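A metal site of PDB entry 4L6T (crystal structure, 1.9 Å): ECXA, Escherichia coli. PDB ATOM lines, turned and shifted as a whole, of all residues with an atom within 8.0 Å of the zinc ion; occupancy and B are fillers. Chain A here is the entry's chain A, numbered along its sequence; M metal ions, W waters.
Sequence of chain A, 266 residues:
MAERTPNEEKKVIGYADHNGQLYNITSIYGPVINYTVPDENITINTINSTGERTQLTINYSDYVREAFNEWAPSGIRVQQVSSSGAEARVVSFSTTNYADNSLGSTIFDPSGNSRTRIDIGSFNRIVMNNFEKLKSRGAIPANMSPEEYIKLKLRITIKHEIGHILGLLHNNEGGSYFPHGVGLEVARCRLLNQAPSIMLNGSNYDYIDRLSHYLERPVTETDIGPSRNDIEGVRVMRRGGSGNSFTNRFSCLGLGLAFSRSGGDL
SD of Met 199 is in hydrogen-bond range of ND1 of His 160 (3.8 Å).
A ring nitrogen (ND1) of His 160 lies within hydrogen-bond range of the backbone carbonyl oxygen of Ile 198 (2.8 Å).
The backbone carbonyl oxygen (O) of Leu 168 sits at hydrogen-bond distance from a ring nitrogen (ND1) of His 164, 2.8 Å away.
A ring nitrogen (ND1) of His 170 sits at hydrogen-bond distance from the side-chain carboxylate of Glu 173.
The zinc ion is bound by a ring nitrogen (NE2) of His 160, a ring nitrogen (NE2) of His 164, a ring nitrogen (NE2) of His 170 and water W1.
The zinc ion has four donor atoms within binding distance.
Within 4 Å of the zinc ion: His 160, His 164 and His 170.
The nearest printed residue that does not touch the zinc ion is Glu 161 (4.6 Å).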
ATOM      1  N   GLY A 104       1.955   6.801  19.663  1.00  0.00           N
ATOM      2  CA  GLY A 104       2.713   5.781  18.974  1.00  0.00           C
ATOM      3  C   GLY A 104       3.722   6.392  18.017  1.00  0.00           C
ATOM      4  O   GLY A 104       3.589   7.549  17.620  1.00  0.00           O
ATOM      5  N   SER A 105       4.714   5.602  17.633  1.00  0.00           N
ATOM      6  CA  SER A 105       5.773   6.083  16.763  1.00  0.00           C
ATOM      7  C   SER A 105       6.463   4.909  16.071  1.00  0.00           C
ATOM      8  O   SER A 105       6.509   3.807  16.609  1.00  0.00           O
ATOM      9  CB  SER A 105       6.787   6.908  17.564  1.00  0.00           C
ATOM     10  OG  SER A 105       7.888   7.307  16.753  1.00  0.00           O
ATOM     11  N   THR A 106       6.983   5.143  14.871  1.00  0.00           N
ATOM     12  CA  THR A 106       7.622   4.082  14.093  1.00  0.00           C
ATOM     13  C   THR A 106       8.890   4.566  13.400  1.00  0.00           C
ATOM     14  O   THR A 106       8.927   5.657  12.838  1.00  0.00           O
ATOM     15  CB  THR A 106       6.652   3.501  13.028  1.00  0.00           C
ATOM     16  OG1 THR A 106       5.550   2.868  13.684  1.00  0.00           O
ATOM     17  CG2 THR A 106       7.352   2.487  12.141  1.00  0.00           C
ATOM     18  N   THR A 157      -4.164   3.490  16.355  1.00  0.00           N
ATOM     19  CA  THR A 157      -2.732   3.753  16.521  1.00  0.00           C
ATOM     20  C   THR A 157      -1.864   2.640  15.929  1.00  0.00           C
ATOM     21  O   THR A 157      -0.889   2.925  15.238  1.00  0.00           O
ATOM     22  CB  THR A 157      -2.374   3.936  18.018  1.00  0.00           C
ATOM     23  OG1 THR A 157      -3.100   5.043  18.548  1.00  0.00           O
ATOM     24  CG2 THR A 157      -0.885   4.180  18.187  1.00  0.00           C
ATOM     25  N   HIS A 160      -2.227   2.390  12.091  1.00  0.00           N
ATOM     26  CA  HIS A 160      -1.556   3.564  11.546  1.00  0.00           C
ATOM     27  C   HIS A 160      -0.036   3.376  11.539  1.00  0.00           C
ATOM     28  O   HIS A 160       0.636   3.690  10.559  1.00  0.00           O
ATOM     29  CB  HIS A 160      -1.949   4.812  12.345  1.00  0.00           C
ATOM     30  CG  HIS A 160      -1.146   6.034  12.001  1.00  0.00           C
ATOM     31  ND1 HIS A 160      -1.543   6.941  11.051  1.00  0.00           N
ATOM     32  CD2 HIS A 160       0.026   6.500  12.512  1.00  0.00           C
ATOM     33  CE1 HIS A 160      -0.647   7.917  10.966  1.00  0.00           C
ATOM     34  NE2 HIS A 160       0.305   7.665  11.852  1.00  0.00           N
ATOM     35  N   GLU A 161       0.522   2.852  12.636  1.00  0.00           N
ATOM     36  CA  GLU A 161       1.954   2.611  12.686  1.00  0.00           C
ATOM     37  C   GLU A 161       2.343   1.489  11.714  1.00  0.00           C
ATOM     38  O   GLU A 161       3.416   1.531  11.115  1.00  0.00           O
ATOM     39  CB  GLU A 161       2.407   2.275  14.113  1.00  0.00           C
ATOM     40  CG  GLU A 161       2.159   3.383  15.130  1.00  0.00           C
ATOM     41  CD  GLU A 161       2.767   4.719  14.741  1.00  0.00           C
ATOM     42  OE1 GLU A 161       3.821   4.736  14.080  1.00  0.00           O
ATOM     43  OE2 GLU A 161       2.171   5.766  15.093  1.00  0.00           O
ATOM     44  N   GLY A 163       1.071   1.056   8.890  1.00  0.00           N
ATOM     45  CA  GLY A 163       1.209   1.797   7.647  1.00  0.00           C
ATOM     46  C   GLY A 163       2.624   2.309   7.467  1.00  0.00           C
ATOM     47  O   GLY A 163       3.199   2.196   6.378  1.00  0.00           O
ATOM     48  N   HIS A 164       3.212   2.854   8.529  1.00  0.00           N
ATOM     49  CA  HIS A 164       4.578   3.346   8.480  1.00  0.00           C
ATOM     50  C   HIS A 164       5.543   2.178   8.235  1.00  0.00           C
ATOM     51  O   HIS A 164       6.506   2.314   7.474  1.00  0.00           O
ATOM     52  CB  HIS A 164       4.951   4.085   9.777  1.00  0.00           C
ATOM     53  CG  HIS A 164       4.318   5.432   9.904  1.00  0.00           C
ATOM     54  ND1 HIS A 164       4.178   6.300   8.854  1.00  0.00           N
ATOM     55  CD2 HIS A 164       3.784   6.065  10.981  1.00  0.00           C
ATOM     56  CE1 HIS A 164       3.588   7.415   9.258  1.00  0.00           C
ATOM     57  NE2 HIS A 164       3.337   7.288  10.558  1.00  0.00           N
ATOM     58  N   LEU A 168       4.566   3.687   4.230  1.00  0.00           N
ATOM     59  CA  LEU A 168       3.750   4.885   4.068  1.00  0.00           C
ATOM     60  C   LEU A 168       4.170   6.008   5.021  1.00  0.00           C
ATOM     61  O   LEU A 168       4.644   5.752   6.124  1.00  0.00           O
ATOM     62  CB  LEU A 168       2.269   4.568   4.275  1.00  0.00           C
ATOM     63  CG  LEU A 168       1.674   3.532   3.315  1.00  0.00           C
ATOM     64  CD1 LEU A 168       0.152   3.550   3.387  1.00  0.00           C
ATOM     65  CD2 LEU A 168       2.161   3.781   1.891  1.00  0.00           C
ATOM     66  N   LEU A 169       3.967   7.240   4.575  1.00  0.00           N
ATOM     67  CA  LEU A 169       4.147   8.416   5.416  1.00  0.00           C
ATOM     68  C   LEU A 169       2.780   9.063   5.625  1.00  0.00           C
ATOM     69  O   LEU A 169       1.752   8.419   5.424  1.00  0.00           O
ATOM     70  CB  LEU A 169       5.143   9.384   4.787  1.00  0.00           C
ATOM     71  CG  LEU A 169       6.548   8.802   4.603  1.00  0.00           C
ATOM     72  CD1 LEU A 169       7.314   9.588   3.570  1.00  0.00           C
ATOM     73  CD2 LEU A 169       7.300   8.754   5.924  1.00  0.00           C
ATOM     74  N   HIS A 170       2.748  10.334   6.034  1.00  0.00           N
ATOM     75  CA  HIS A 170       1.466  11.016   6.250  1.00  0.00           C
ATOM     76  C   HIS A 170       0.936  11.645   4.966  1.00  0.00           C
ATOM     77  O   HIS A 170       1.709  11.944   4.060  1.00  0.00           O
ATOM     78  CB  HIS A 170       1.588  12.090   7.321  1.00  0.00           C
ATOM     79  CG  HIS A 170       1.985  11.554   8.655  1.00  0.00           C
ATOM     80  ND1 HIS A 170       2.949  12.148   9.441  1.00  0.00           N
ATOM     81  CD2 HIS A 170       1.550  10.474   9.341  1.00  0.00           C
ATOM     82  CE1 HIS A 170       3.084  11.459  10.558  1.00  0.00           C
ATOM     83  NE2 HIS A 170       2.252  10.436  10.527  1.00  0.00           N
ATOM     84  N   ASN A 171      -0.376  11.852   4.907  1.00  0.00           N
ATOM     85  CA  ASN A 171      -1.034  12.357   3.698  1.00  0.00           C
ATOM     86  C   ASN A 171      -0.468  13.672   3.187  1.00  0.00           C
ATOM     87  O   ASN A 171      -0.485  13.945   1.979  1.00  0.00           O
ATOM     88  CB  ASN A 171      -2.528  12.525   3.945  1.00  0.00           C
ATOM     89  CG  ASN A 171      -2.834  13.695   4.875  1.00  0.00           C
ATOM     90  OD1 ASN A 171      -2.222  13.829   5.934  1.00  0.00           O
ATOM     91  ND2 ASN A 171      -3.775  14.541   4.475  1.00  0.00           N
ATOM     92  N   GLU A 173       2.673  14.832   3.504  1.00  0.00           N
ATOM     93  CA  GLU A 173       4.138  14.872   3.553  1.00  0.00           C
ATOM     94  C   GLU A 173       4.789  14.620   2.191  1.00  0.00           C
ATOM     95  O   GLU A 173       5.979  14.326   2.132  1.00  0.00           O
ATOM     96  CB  GLU A 173       4.641  13.879   4.596  1.00  0.00           C
ATOM     97  CG  GLU A 173       4.465  14.415   6.013  1.00  0.00           C
ATOM     98  CD  GLU A 173       4.731  13.383   7.090  1.00  0.00           C
ATOM     99  OE1 GLU A 173       4.873  12.188   6.764  1.00  0.00           O
ATOM    100  OE2 GLU A 173       4.790  13.776   8.277  1.00  0.00           O
ATOM    101  N   ILE A 198      -6.126   6.222   6.758  1.00  0.00           N
ATOM    102  CA  ILE A 198      -5.760   6.062   8.159  1.00  0.00           C
ATOM    103  C   ILE A 198      -4.369   6.661   8.405  1.00  0.00           C
ATOM    104  O   ILE A 198      -3.895   6.754   9.538  1.00  0.00           O
ATOM    105  CB  ILE A 198      -5.812   4.574   8.582  1.00  0.00           C
ATOM    106  CG1 ILE A 198      -5.806   4.442  10.115  1.00  0.00           C
ATOM    107  CG2 ILE A 198      -4.678   3.782   7.927  1.00  0.00           C
ATOM    108  CD1 ILE A 198      -6.118   3.052  10.606  1.00  0.00           C
ATOM    109  N   MET A 199      -3.714   7.085   7.325  1.00  0.00           N
ATOM    110  CA  MET A 199      -2.395   7.691   7.434  1.00  0.00           C
ATOM    111  C   MET A 199      -2.458   9.220   7.437  1.00  0.00           C
ATOM    112  O   MET A 199      -1.451   9.876   7.188  1.00  0.00           O
ATOM    113  CB  MET A 199      -1.486   7.201   6.316  1.00  0.00           C
ATOM    114  CG  MET A 199      -1.325   5.694   6.283  1.00  0.00           C
ATOM    115  SD  MET A 199      -0.806   5.031   7.884  1.00  0.00           S
ATOM    116  CE  MET A 199       0.817   5.775   8.066  1.00  0.00           C
ATOM    117  N   LEU A 200      -3.650   9.766   7.688  1.00  0.00           N
ATOM    118  CA  LEU A 200      -3.785  11.207   7.944  1.00  0.00           C
ATOM    119  C   LEU A 200      -2.767  11.666   8.973  1.00  0.00           C
ATOM    120  O   LEU A 200      -2.525  10.971   9.954  1.00  0.00           O
ATOM    121  CB  LEU A 200      -5.192  11.544   8.441  1.00  0.00           C
ATOM    122  CG  LEU A 200      -6.368  11.438   7.465  1.00  0.00           C
ATOM    123  CD1 LEU A 200      -7.654  11.901   8.140  1.00  0.00           C
ATOM    124  CD2 LEU A 200      -6.097  12.244   6.193  1.00  0.00           C
ATOM    125  N   ASN A 201      -2.175  12.843   8.738  1.00  0.00           N
ATOM    126  CA  ASN A 201      -1.230  13.418   9.699  1.00  0.00           C
ATOM    127  C   ASN A 201      -1.974  13.777  10.982  1.00  0.00           C
ATOM    128  O   ASN A 201      -2.827  14.668  10.992  1.00  0.00           O
ATOM    129  CB  ASN A 201      -0.527  14.647   9.107  1.00  0.00           C
ATOM    130  CG  ASN A 201       0.725  15.038   9.874  1.00  0.00           C
ATOM    131  OD1 ASN A 201       0.775  14.924  11.097  1.00  0.00           O
ATOM    132  ND2 ASN A 201       1.753  15.497   9.166  1.00  0.00           N
ATOM    133  N   GLY A 202      -1.636  13.080  12.054  1.00  0.00           N
ATOM    134  CA  GLY A 202      -2.301  13.248  13.335  1.00  0.00           C
ATOM    135  C   GLY A 202      -2.108  14.631  13.946  1.00  0.00           C
ATOM    136  O   GLY A 202      -2.887  15.039  14.813  1.00  0.00           O
ATOM    137  N   SER A 203      -1.082  15.341  13.495  1.00  0.00           N
ATOM    138  CA  SER A 203      -0.872  16.713  13.965  1.00  0.00           C
ATOM    139  C   SER A 203      -1.915  17.653  13.379  1.00  0.00           C
ATOM    140  O   SER A 203      -2.202  18.700  13.947  1.00  0.00           O
ATOM    141  CB  SER A 203       0.536  17.201  13.584  1.00  0.00           C
ATOM    142  OG  SER A 203       1.532  16.526  14.328  1.00  0.00           O
HETATM  143 ZN    ZN M   1       2.096   8.612  11.538  1.00  0.00          ZN
HETATM  144  O   HOH W   1       3.101   8.713  13.869  1.00  0.00           O
HETATM  145  O   HOH W   2      -0.272  10.686  12.924  1.00  0.00           O
